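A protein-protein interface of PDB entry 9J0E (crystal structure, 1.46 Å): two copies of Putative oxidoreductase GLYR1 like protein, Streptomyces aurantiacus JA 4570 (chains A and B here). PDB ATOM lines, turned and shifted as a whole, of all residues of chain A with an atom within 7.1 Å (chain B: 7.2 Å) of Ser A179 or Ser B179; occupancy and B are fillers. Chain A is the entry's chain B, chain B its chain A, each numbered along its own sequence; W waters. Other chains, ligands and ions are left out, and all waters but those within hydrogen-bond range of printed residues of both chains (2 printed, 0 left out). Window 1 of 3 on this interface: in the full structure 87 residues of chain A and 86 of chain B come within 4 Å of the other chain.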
ATOM      1  N   LEU A 173      18.121  14.596  19.689  1.00  0.00           N
ATOM      2  CA  LEU A 173      17.665  15.177  20.946  1.00  0.00           C
ATOM      3  C   LEU A 173      17.252  14.096  21.937  1.00  0.00           C
ATOM      4  O   LEU A 173      17.398  14.282  23.150  1.00  0.00           O
ATOM      5  CB  LEU A 173      16.508  16.139  20.711  1.00  0.00           C
ATOM      6  CG  LEU A 173      16.776  17.404  19.907  1.00  0.00           C
ATOM      7  CD1 LEU A 173      15.489  18.198  19.827  1.00  0.00           C
ATOM      8  CD2 LEU A 173      17.861  18.224  20.583  1.00  0.00           C
ATOM      9  N   ASP A 174      16.716  12.980  21.444  1.00  0.00           N
ATOM     10  CA  ASP A 174      16.451  11.830  22.301  1.00  0.00           C
ATOM     11  C   ASP A 174      17.709  11.456  23.077  1.00  0.00           C
ATOM     12  O   ASP A 174      17.701  11.372  24.312  1.00  0.00           O
ATOM     13  CB  ASP A 174      15.995  10.681  21.390  1.00  0.00           C
ATOM     14  CG  ASP A 174      15.347   9.516  22.134  1.00  0.00           C
ATOM     15  OD1 ASP A 174      15.447   9.420  23.373  1.00  0.00           O
ATOM     16  OD2 ASP A 174      14.732   8.675  21.433  1.00  0.00           O
ATOM     17  N   PHE A 175      18.815  11.263  22.364  1.00  0.00           N
ATOM     18  CA  PHE A 175      20.086  10.986  23.022  1.00  0.00           C
ATOM     19  C   PHE A 175      20.499  12.127  23.947  1.00  0.00           C
ATOM     20  O   PHE A 175      20.888  11.898  25.098  1.00  0.00           O
ATOM     21  CB  PHE A 175      21.166  10.729  21.968  1.00  0.00           C
ATOM     22  CG  PHE A 175      22.552  10.751  22.521  1.00  0.00           C
ATOM     23  CD1 PHE A 175      23.015   9.705  23.308  1.00  0.00           C
ATOM     24  CD2 PHE A 175      23.392  11.822  22.274  1.00  0.00           C
ATOM     25  CE1 PHE A 175      24.283   9.721  23.825  1.00  0.00           C
ATOM     26  CE2 PHE A 175      24.678  11.855  22.796  1.00  0.00           C
ATOM     27  CZ  PHE A 175      25.128  10.799  23.579  1.00  0.00           C
ATOM     28  N   LEU A 176      20.440  13.367  23.457  1.00  0.00           N
ATOM     29  CA  LEU A 176      21.011  14.484  24.206  1.00  0.00           C
ATOM     30  C   LEU A 176      20.266  14.736  25.515  1.00  0.00           C
ATOM     31  O   LEU A 176      20.891  14.842  26.583  1.00  0.00           O
ATOM     32  CB  LEU A 176      21.023  15.740  23.333  1.00  0.00           C
ATOM     33  CG  LEU A 176      21.609  16.971  24.029  1.00  0.00           C
ATOM     34  CD1 LEU A 176      23.075  16.757  24.339  1.00  0.00           C
ATOM     35  CD2 LEU A 176      21.424  18.174  23.116  1.00  0.00           C
ATOM     36  N   PHE A 177      18.934  14.848  25.455  1.00  0.00           N
ATOM     37  CA  PHE A 177      18.157  15.117  26.661  1.00  0.00           C
ATOM     38  C   PHE A 177      18.204  13.946  27.636  1.00  0.00           C
ATOM     39  O   PHE A 177      18.265  14.151  28.853  1.00  0.00           O
ATOM     40  CB  PHE A 177      16.705  15.465  26.319  1.00  0.00           C
ATOM     41  CG  PHE A 177      16.501  16.895  25.913  1.00  0.00           C
ATOM     42  CD1 PHE A 177      15.909  17.202  24.699  1.00  0.00           C
ATOM     43  CD2 PHE A 177      16.902  17.930  26.747  1.00  0.00           C
ATOM     44  CE1 PHE A 177      15.724  18.527  24.319  1.00  0.00           C
ATOM     45  CE2 PHE A 177      16.721  19.256  26.378  1.00  0.00           C
ATOM     46  CZ  PHE A 177      16.131  19.553  25.163  1.00  0.00           C
ATOM     47  N   THR A 178      18.162  12.712  27.133  1.00  0.00           N
ATOM     48  CA  THR A 178      18.324  11.575  28.032  1.00  0.00           C
ATOM     49  C   THR A 178      19.681  11.617  28.731  1.00  0.00           C
ATOM     50  O   THR A 178      19.764  11.427  29.951  1.00  0.00           O
ATOM     51  CB  THR A 178      18.109  10.274  27.261  1.00  0.00           C
ATOM     52  OG1 THR A 178      16.799  10.294  26.677  1.00  0.00           O
ATOM     53  CG2 THR A 178      18.218   9.061  28.199  1.00  0.00           C
ATOM     54  N   SER A 179      20.750  11.900  27.981  1.00  0.00           N
ATOM     55  CA  SER A 179      22.078  12.010  28.580  1.00  0.00           C
ATOM     56  C   SER A 179      22.133  13.140  29.599  1.00  0.00           C
ATOM     57  O   SER A 179      22.701  12.973  30.689  1.00  0.00           O
ATOM     58  CB  SER A 179      23.112  12.243  27.484  1.00  0.00           C
ATOM     59  OG  SER A 179      23.159  11.154  26.580  1.00  0.00           O
ATOM     60  N   MET A 180      21.555  14.301  29.259  1.00  0.00           N
ATOM     61  CA  MET A 180      21.569  15.435  30.184  1.00  0.00           C
ATOM     62  C   MET A 180      20.820  15.112  31.472  1.00  0.00           C
ATOM     63  O   MET A 180      21.231  15.533  32.561  1.00  0.00           O
ATOM     64  CB  MET A 180      20.975  16.675  29.510  1.00  0.00           C
ATOM     65  CG  MET A 180      21.871  17.311  28.443  1.00  0.00           C
ATOM     66  SD  MET A 180      20.968  18.484  27.368  1.00  0.00           S
ATOM     67  CE  MET A 180      20.574  19.809  28.519  1.00  0.00           C
ATOM     68  N   SER A 181      19.725  14.351  31.373  1.00  0.00           N
ATOM     69  CA  SER A 181      19.030  13.893  32.575  1.00  0.00           C
ATOM     70  C   SER A 181      19.951  13.036  33.438  1.00  0.00           C
ATOM     71  O   SER A 181      20.011  13.211  34.662  1.00  0.00           O
ATOM     72  CB  SER A 181      17.761  13.125  32.190  1.00  0.00           C
ATOM     73  OG  SER A 181      17.983  11.736  32.038  1.00  0.00           O
ATOM     74  N   GLY A 182      20.691  12.117  32.812  1.00  0.00           N
ATOM     75  CA  GLY A 182      21.609  11.264  33.556  1.00  0.00           C
ATOM     76  C   GLY A 182      22.769  12.014  34.183  1.00  0.00           C
ATOM     77  O   GLY A 182      23.260  11.628  35.249  1.00  0.00           O
ATOM     78  N   LEU A 183      23.230  13.086  33.535  1.00  0.00           N
ATOM     79  CA  LEU A 183      24.313  13.884  34.094  1.00  0.00           C
ATOM     80  C   LEU A 183      23.859  14.587  35.368  1.00  0.00           C
ATOM     81  O   LEU A 183      24.550  14.547  36.397  1.00  0.00           O
ATOM     82  CB  LEU A 183      24.775  14.895  33.043  1.00  0.00           C
ATOM     83  CG  LEU A 183      25.904  15.836  33.472  1.00  0.00           C
ATOM     84  CD1 LEU A 183      27.169  15.045  33.789  1.00  0.00           C
ATOM     85  CD2 LEU A 183      26.144  16.873  32.384  1.00  0.00           C
ATOM     86  N   VAL A 184      22.695  15.239  35.311  1.00  0.00           N
ATOM     87  CA  VAL A 184      22.117  15.862  36.499  1.00  0.00           C
ATOM     88  C   VAL A 184      21.880  14.819  37.580  1.00  0.00           C
ATOM     89  O   VAL A 184      22.164  15.051  38.759  1.00  0.00           O
ATOM     90  CB  VAL A 184      20.827  16.614  36.117  1.00  0.00           C
ATOM     91  CG1 VAL A 184      19.999  16.958  37.344  1.00  0.00           C
ATOM     92  CG2 VAL A 184      21.146  17.861  35.265  1.00  0.00           C
ATOM     93  N   HIS A 185      21.362  13.653  37.194  1.00  0.00           N
ATOM     94  CA  HIS A 185      21.027  12.632  38.180  1.00  0.00           C
ATOM     95  C   HIS A 185      22.271  12.100  38.872  1.00  0.00           C
ATOM     96  O   HIS A 185      22.276  11.926  40.099  1.00  0.00           O
ATOM     97  CB  HIS A 185      20.243  11.494  37.523  1.00  0.00           C
ATOM     98  CG  HIS A 185      19.400  10.725  38.488  1.00  0.00           C
ATOM     99  ND1 HIS A 185      19.880   9.647  39.200  1.00  0.00           N
ATOM    100  CD2 HIS A 185      18.120  10.904  38.891  1.00  0.00           C
ATOM    101  CE1 HIS A 185      18.923   9.182  39.986  1.00  0.00           C
ATOM    102  NE2 HIS A 185      17.846   9.928  39.819  1.00  0.00           N
ATOM    103  N   ILE A 208      32.834  10.348  28.664  1.00  0.00           N
ATOM    104  CA  ILE A 208      32.592  11.017  27.390  1.00  0.00           C
ATOM    105  C   ILE A 208      33.366  10.321  26.282  1.00  0.00           C
ATOM    106  O   ILE A 208      32.837  10.085  25.189  1.00  0.00           O
ATOM    107  CB  ILE A 208      32.949  12.510  27.481  1.00  0.00           C
ATOM    108  CG1 ILE A 208      32.126  13.222  28.559  1.00  0.00           C
ATOM    109  CG2 ILE A 208      32.729  13.161  26.127  1.00  0.00           C
ATOM    110  CD1 ILE A 208      30.643  13.215  28.312  1.00  0.00           C
ATOM    111  N   LEU A 211      31.588   7.203  25.409  1.00  0.00           N
ATOM    112  CA  LEU A 211      30.397   7.477  24.614  1.00  0.00           C
ATOM    113  C   LEU A 211      30.760   7.833  23.185  1.00  0.00           C
ATOM    114  O   LEU A 211      30.032   7.473  22.253  1.00  0.00           O
ATOM    115  CB  LEU A 211      29.564   8.585  25.255  1.00  0.00           C
ATOM    116  CG  LEU A 211      28.774   8.187  26.500  1.00  0.00           C
ATOM    117  CD1 LEU A 211      28.279   9.429  27.233  1.00  0.00           C
ATOM    118  CD2 LEU A 211      27.603   7.290  26.112  1.00  0.00           C
ATOM    119  N   VAL A 261      15.298   2.792  32.315  1.00  0.00           N
ATOM    120  CA  VAL A 261      16.527   2.226  31.766  1.00  0.00           C
ATOM    121  C   VAL A 261      16.591   0.742  32.071  1.00  0.00           C
ATOM    122  O   VAL A 261      16.840  -0.093  31.189  1.00  0.00           O
ATOM    123  CB  VAL A 261      17.751   2.962  32.336  1.00  0.00           C
ATOM    124  CG1 VAL A 261      19.028   2.281  31.877  1.00  0.00           C
ATOM    125  CG2 VAL A 261      17.736   4.439  31.909  1.00  0.00           C
ATOM    126  N   TRP A 278      24.969  -4.344  25.536  1.00  0.00           N
ATOM    127  CA  TRP A 278      23.964  -3.308  25.748  1.00  0.00           C
ATOM    128  C   TRP A 278      23.178  -2.995  24.480  1.00  0.00           C
ATOM    129  O   TRP A 278      22.006  -2.601  24.551  1.00  0.00           O
ATOM    130  CB  TRP A 278      24.620  -2.019  26.266  1.00  0.00           C
ATOM    131  CG  TRP A 278      23.599  -0.966  26.531  1.00  0.00           C
ATOM    132  CD1 TRP A 278      23.268   0.091  25.730  1.00  0.00           C
ATOM    133  CD2 TRP A 278      22.743  -0.892  27.672  1.00  0.00           C
ATOM    134  NE1 TRP A 278      22.243   0.810  26.300  1.00  0.00           N
ATOM    135  CE2 TRP A 278      21.904   0.226  27.494  1.00  0.00           C
ATOM    136  CE3 TRP A 278      22.591  -1.682  28.820  1.00  0.00           C
ATOM    137  CZ2 TRP A 278      20.937   0.591  28.435  1.00  0.00           C
ATOM    138  CZ3 TRP A 278      21.634  -1.320  29.753  1.00  0.00           C
ATOM    139  CH2 TRP A 278      20.818  -0.196  29.556  1.00  0.00           C
ATOM    140  N   LEU B 173      28.279   5.876  36.627  1.00  0.00           N
ATOM    141  CA  LEU B 173      27.491   4.883  35.897  1.00  0.00           C
ATOM    142  C   LEU B 173      26.060   5.346  35.682  1.00  0.00           C
ATOM    143  O   LEU B 173      25.444   4.987  34.674  1.00  0.00           O
ATOM    144  CB  LEU B 173      27.491   3.542  36.629  1.00  0.00           C
ATOM    145  CG  LEU B 173      28.824   2.806  36.755  1.00  0.00           C
ATOM    146  CD1 LEU B 173      28.590   1.504  37.505  1.00  0.00           C
ATOM    147  CD2 LEU B 173      29.437   2.524  35.407  1.00  0.00           C
ATOM    148  N   ASP B 174      25.503   6.103  36.629  1.00  0.00           N
ATOM    149  CA  ASP B 174      24.197   6.723  36.437  1.00  0.00           C
ATOM    150  C   ASP B 174      24.185   7.508  35.126  1.00  0.00           C
ATOM    151  O   ASP B 174      23.336   7.289  34.243  1.00  0.00           O
ATOM    152  CB  ASP B 174      23.944   7.634  37.648  1.00  0.00           C
ATOM    153  CG  ASP B 174      22.513   8.124  37.775  1.00  0.00           C
ATOM    154  OD1 ASP B 174      21.699   7.997  36.826  1.00  0.00           O
ATOM    155  OD2 ASP B 174      22.207   8.662  38.869  1.00  0.00           O
ATOM    156  N   PHE B 175      25.157   8.402  34.968  1.00  0.00           N
ATOM    157  CA  PHE B 175      25.284   9.147  33.725  1.00  0.00           C
ATOM    158  C   PHE B 175      25.499   8.214  32.538  1.00  0.00           C
ATOM    159  O   PHE B 175      24.838   8.353  31.499  1.00  0.00           O
ATOM    160  CB  PHE B 175      26.444  10.137  33.843  1.00  0.00           C
ATOM    161  CG  PHE B 175      26.868  10.714  32.524  1.00  0.00           C
ATOM    162  CD1 PHE B 175      26.048  11.613  31.865  1.00  0.00           C
ATOM    163  CD2 PHE B 175      28.073  10.344  31.938  1.00  0.00           C
ATOM    164  CE1 PHE B 175      26.426  12.154  30.644  1.00  0.00           C
ATOM    165  CE2 PHE B 175      28.456  10.880  30.719  1.00  0.00           C
ATOM    166  CZ  PHE B 175      27.627  11.790  30.073  1.00  0.00           C
ATOM    167  N   LEU B 176      26.434   7.265  32.664  1.00  0.00           N
ATOM    168  CA  LEU B 176      26.821   6.465  31.503  1.00  0.00           C
ATOM    169  C   LEU B 176      25.672   5.583  31.019  1.00  0.00           C
ATOM    170  O   LEU B 176      25.351   5.572  29.824  1.00  0.00           O
ATOM    171  CB  LEU B 176      28.064   5.630  31.812  1.00  0.00           C
ATOM    172  CG  LEU B 176      28.530   4.710  30.671  1.00  0.00           C
ATOM    173  CD1 LEU B 176      28.997   5.517  29.471  1.00  0.00           C
ATOM    174  CD2 LEU B 176      29.639   3.778  31.141  1.00  0.00           C
ATOM    175  N   PHE B 177      25.055   4.811  31.924  1.00  0.00           N
ATOM    176  CA  PHE B 177      23.967   3.927  31.499  1.00  0.00           C
ATOM    177  C   PHE B 177      22.760   4.709  30.997  1.00  0.00           C
ATOM    178  O   PHE B 177      22.115   4.308  30.017  1.00  0.00           O
ATOM    179  CB  PHE B 177      23.558   2.984  32.626  1.00  0.00           C
ATOM    180  CG  PHE B 177      24.433   1.781  32.751  1.00  0.00           C
ATOM    181  CD1 PHE B 177      25.063   1.490  33.957  1.00  0.00           C
ATOM    182  CD2 PHE B 177      24.615   0.927  31.670  1.00  0.00           C
ATOM    183  CE1 PHE B 177      25.870   0.372  34.082  1.00  0.00           C
ATOM    184  CE2 PHE B 177      25.426  -0.190  31.784  1.00  0.00           C
ATOM    185  CZ  PHE B 177      26.050  -0.468  32.990  1.00  0.00           C
ATOM    186  N   THR B 178      22.425   5.825  31.651  1.00  0.00           N
ATOM    187  CA  THR B 178      21.307   6.626  31.168  1.00  0.00           C
ATOM    188  C   THR B 178      21.596   7.143  29.761  1.00  0.00           C
ATOM    189  O   THR B 178      20.724   7.106  28.878  1.00  0.00           O
ATOM    190  CB  THR B 178      21.027   7.775  32.149  1.00  0.00           C
ATOM    191  OG1 THR B 178      20.689   7.226  33.432  1.00  0.00           O
ATOM    192  CG2 THR B 178      19.860   8.626  31.679  1.00  0.00           C
ATOM    193  N   SER B 179      22.839   7.581  29.523  1.00  0.00           N
ATOM    194  CA  SER B 179      23.247   8.051  28.200  1.00  0.00           C
ATOM    195  C   SER B 179      23.211   6.925  27.171  1.00  0.00           C
ATOM    196  O   SER B 179      22.716   7.118  26.055  1.00  0.00           O
ATOM    197  CB  SER B 179      24.646   8.649  28.283  1.00  0.00           C
ATOM    198  OG  SER B 179      24.643   9.837  29.060  1.00  0.00           O
ATOM    199  N   MET B 180      23.728   5.741  27.531  1.00  0.00           N
ATOM    200  CA  MET B 180      23.676   4.608  26.609  1.00  0.00           C
ATOM    201  C   MET B 180      22.241   4.224  26.278  1.00  0.00           C
ATOM    202  O   MET B 180      21.961   3.804  25.149  1.00  0.00           O
ATOM    203  CB  MET B 180      24.444   3.419  27.192  1.00  0.00           C
ATOM    204  CG  MET B 180      25.960   3.632  27.280  1.00  0.00           C
ATOM    205  SD  MET B 180      26.770   2.397  28.338  1.00  0.00           S
ATOM    206  CE  MET B 180      26.635   0.908  27.351  1.00  0.00           C
ATOM    207  N   SER B 181      21.323   4.358  27.241  1.00  0.00           N
ATOM    208  CA  SER B 181      19.908   4.111  26.969  1.00  0.00           C
ATOM    209  C   SER B 181      19.387   5.074  25.907  1.00  0.00           C
ATOM    210  O   SER B 181      18.714   4.667  24.949  1.00  0.00           O
ATOM    211  CB  SER B 181      19.113   4.253  28.271  1.00  0.00           C
ATOM    212  OG  SER B 181      17.730   4.004  28.084  1.00  0.00           O
ATOM    213  N   GLY B 182      19.700   6.363  26.063  1.00  0.00           N
ATOM    214  CA  GLY B 182      19.258   7.361  25.104  1.00  0.00           C
ATOM    215  C   GLY B 182      19.885   7.195  23.736  1.00  0.00           C
ATOM    216  O   GLY B 182      19.250   7.498  22.723  1.00  0.00           O
ATOM    217  N   LEU B 183      21.128   6.708  23.684  1.00  0.00           N
ATOM    218  CA  LEU B 183      21.776   6.458  22.400  1.00  0.00           C
ATOM    219  C   LEU B 183      21.043   5.371  21.619  1.00  0.00           C
ATOM    220  O   LEU B 183      20.695   5.563  20.449  1.00  0.00           O
ATOM    221  CB  LEU B 183      23.242   6.078  22.620  1.00  0.00           C
ATOM    222  CG  LEU B 183      24.045   5.793  21.348  1.00  0.00           C
ATOM    223  CD1 LEU B 183      24.150   7.053  20.483  1.00  0.00           C
ATOM    224  CD2 LEU B 183      25.442   5.263  21.701  1.00  0.00           C
ATOM    225  N   VAL B 184      20.809   4.218  22.257  1.00  0.00           N
ATOM    226  CA  VAL B 184      20.004   3.154  21.653  1.00  0.00           C
ATOM    227  C   VAL B 184      18.630   3.678  21.253  1.00  0.00           C
ATOM    228  O   VAL B 184      18.117   3.364  20.167  1.00  0.00           O
ATOM    229  CB  VAL B 184      19.897   1.966  22.631  1.00  0.00           C
ATOM    230  CG1 VAL B 184      18.837   0.978  22.142  1.00  0.00           C
ATOM    231  CG2 VAL B 184      21.228   1.262  22.755  1.00  0.00           C
ATOM    232  N   HIS B 185      18.002   4.469  22.123  1.00  0.00           N
ATOM    233  CA  HIS B 185      16.632   4.904  21.873  1.00  0.00           C
ATOM    234  C   HIS B 185      16.553   5.848  20.684  1.00  0.00           C
ATOM    235  O   HIS B 185      15.648   5.725  19.848  1.00  0.00           O
ATOM    236  CB  HIS B 185      16.039   5.558  23.119  1.00  0.00           C
ATOM    237  CG  HIS B 185      14.544   5.568  23.130  1.00  0.00           C
ATOM    238  ND1 HIS B 185      13.795   6.565  22.538  1.00  0.00           N
ATOM    239  CD2 HIS B 185      13.655   4.670  23.619  1.00  0.00           C
ATOM    240  CE1 HIS B 185      12.510   6.292  22.687  1.00  0.00           C
ATOM    241  NE2 HIS B 185      12.399   5.148  23.339  1.00  0.00           N
ATOM    242  N   HIS B 207      27.085  16.357  19.558  1.00  0.00           N
ATOM    243  CA  HIS B 207      26.494  16.249  20.882  1.00  0.00           C
ATOM    244  C   HIS B 207      27.465  15.678  21.901  1.00  0.00           C
ATOM    245  O   HIS B 207      27.363  16.003  23.089  1.00  0.00           O
ATOM    246  CB  HIS B 207      25.174  15.482  20.817  1.00  0.00           C
ATOM    247  CG  HIS B 207      24.057  16.314  20.285  1.00  0.00           C
ATOM    248  ND1 HIS B 207      22.761  15.859  20.178  1.00  0.00           N
ATOM    249  CD2 HIS B 207      24.050  17.590  19.831  1.00  0.00           C
ATOM    250  CE1 HIS B 207      22.004  16.817  19.675  1.00  0.00           C
ATOM    251  NE2 HIS B 207      22.762  17.877  19.451  1.00  0.00           N
ATOM    252  N   LEU B 211      28.269  17.581  25.254  1.00  0.00           N
ATOM    253  CA  LEU B 211      28.265  16.952  26.569  1.00  0.00           C
ATOM    254  C   LEU B 211      29.527  17.287  27.357  1.00  0.00           C
ATOM    255  O   LEU B 211      29.463  17.484  28.575  1.00  0.00           O
ATOM    256  CB  LEU B 211      28.058  15.442  26.430  1.00  0.00           C
ATOM    257  CG  LEU B 211      26.609  15.045  26.133  1.00  0.00           C
ATOM    258  CD1 LEU B 211      26.529  13.573  25.721  1.00  0.00           C
ATOM    259  CD2 LEU B 211      25.710  15.314  27.335  1.00  0.00           C
ATOM    260  N   VAL B 261      12.260  11.410  31.978  1.00  0.00           N
ATOM    261  CA  VAL B 261      12.984  12.650  31.697  1.00  0.00           C
ATOM    262  C   VAL B 261      12.018  13.823  31.727  1.00  0.00           C
ATOM    263  O   VAL B 261      12.265  14.848  32.377  1.00  0.00           O
ATOM    264  CB  VAL B 261      13.697  12.551  30.335  1.00  0.00           C
ATOM    265  CG1 VAL B 261      14.327  13.906  29.948  1.00  0.00           C
ATOM    266  CG2 VAL B 261      14.751  11.460  30.364  1.00  0.00           C
ATOM    267  N   TRP B 278      18.437  23.783  32.108  1.00  0.00           N
ATOM    268  CA  TRP B 278      18.265  22.359  32.369  1.00  0.00           C
ATOM    269  C   TRP B 278      18.804  21.955  33.732  1.00  0.00           C
ATOM    270  O   TRP B 278      18.312  20.991  34.335  1.00  0.00           O
ATOM    271  CB  TRP B 278      18.971  21.525  31.297  1.00  0.00           C
ATOM    272  CG  TRP B 278      18.761  20.069  31.532  1.00  0.00           C
ATOM    273  CD1 TRP B 278      19.637  19.193  32.097  1.00  0.00           C
ATOM    274  CD2 TRP B 278      17.573  19.328  31.249  1.00  0.00           C
ATOM    275  NE1 TRP B 278      19.069  17.941  32.176  1.00  0.00           N
ATOM    276  CE2 TRP B 278      17.800  17.998  31.658  1.00  0.00           C
ATOM    277  CE3 TRP B 278      16.338  19.663  30.685  1.00  0.00           C
ATOM    278  CZ2 TRP B 278      16.834  16.999  31.522  1.00  0.00           C
ATOM    279  CZ3 TRP B 278      15.378  18.672  30.544  1.00  0.00           C
ATOM    280  CH2 TRP B 278      15.632  17.353  30.964  1.00  0.00           C
HETATM  281  O   HOH W   1      23.066  10.235  31.048  1.00  0.00           O
HETATM  282  O   HOH W   2      17.124   1.343  28.489  1.00  0.00           O
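Asp A174 touches His B185, and with the chains exchanged His A185 touches Asp B174. Phe A175 touches Gly B182, and with the chains exchanged Gly A182 touches Phe B175. Met A180 touches Trp B278, and with the chains exchanged Trp A278 touches Met B180. Leu A211 touches Ser B179, but with the chains exchanged Ser A179 does not touch Leu B211 (4.03 Å). Of the 27 pairs that touch across the chains among the printed residues, 22 have their exchanged pair printed and touching as well.
Water W1 lies within hydrogen-bond range of OG of Ser B179 (2.6 Å), O of Phe B175 (2.6 Å) and O of Ser A179 (2.8 Å). Water W2 lies within hydrogen-bond range of OG of Ser B181 and O of Val A261.
The side-chain carboxylate (OD2) of Asp B174 is in hydrogen-bond range of a ring nitrogen (ND1) of His A185 (2.5 Å). The side-chain hydroxyl (OG) of Ser B179 sits at hydrogen-bond distance from the side-chain hydroxyl (OG) of Ser A179, 3.2 Å away. O of Met B180 sits at hydrogen-bond distance from NE1 of Trp A278 (3.2 Å). A ring nitrogen (ND1) of His B185 is in hydrogen-bond range of the side-chain carboxylate (OD2) of Asp A174, 2.6 Å away. The indole nitrogen (NE1) of Trp B278 lies within hydrogen-bond range of the backbone carbonyl oxygen (O) of Met A180 (3.3 Å).
Of the 17 printed residues of chain B, 14 touch a printed residue of chain A. Printed residues of chain A that touch a printed residue of chain B: Asp A174, Phe A175, Leu A176, Thr A178, Ser A179, Met A180, Ser A181, Gly A182, Leu A183, Val A184, His A185, Ile A208, Leu A211, Val A261 and Trp A278. Hydrophobic or aromatic side chains of chain A within 4 Å of the printed part of chain B: Phe A175, Leu A176, Met A180, Leu A183, Val A184, His A185, Ile A208, Leu A211, Val A261 and Trp A278. Among the printed residues, no Asp or Glu carboxylate lies within 4 Å of a Lys or Arg side-chain nitrogen of the other chain.
Among the printed residues, merely in contact across the chains: Phe A175 with Ser B179, Phe A175 with Gly B182, Phe A175 with Leu B183, Phe A175 with Leu B211, Leu A176 with His B207, Thr A178 with Thr B178, Thr A178 with Gly B182, Ser A179 with Phe B175, Ser A181 with Thr B178, Ser A181 with Val B261, Ser A181 with Trp B278, Gly A182 with Phe B175, Gly A182 with Thr B178, Leu A183 with Phe B175, Val A184 with Trp B278, Ile A208 with Phe B175, Ile A208 with Leu B211, Leu A211 with Phe B175, Leu A211 with Ser B179, Val A261 with Ser B181, Trp A278 with Ser B181 and Trp A278 with Val B184.
Printed residues of chain B within 4 Å of Val A261: Ser B181 (3.8 Å). Of the printed residues of chain B, Trp A278 touches Met B180, Ser B181 and Val B184. Of the printed residues of chain A, Asp B174 touches His A185 (2.5 Å). Printed residues of chain A within 4 Å of Gly B182: Phe A175 and Thr A178. The nearest residue of chain B that does not touch Ser A179 is Leu B211 (4.03 Å). The nearest residue of chain A that does not touch Ser B179 is Thr A178 (4.9 Å). The nearest printed residue of chain A that does not touch Val B184 is Phe A175 (6.0 Å).
The side-chain hydroxyl (OG1) of Thr B178 lies within hydrogen-bond range of the backbone carbonyl oxygen (O) of Asp B174 (2.8 Å). O of Phe B175 sits at hydrogen-bond distance from OG of Ser B179 (2.9 Å). O of Asp A174 is in hydrogen-bond range of OG1 of Thr A178 (2.8 Å). The backbone carbonyl oxygen of Phe A175 lies within hydrogen-bond range of the side-chain hydroxyl of Ser A179 (2.8 Å). The backbone carbonyl oxygen of Thr A178 is in hydrogen-bond range of the side-chain hydroxyl of Ser A181 (2.8 Å).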
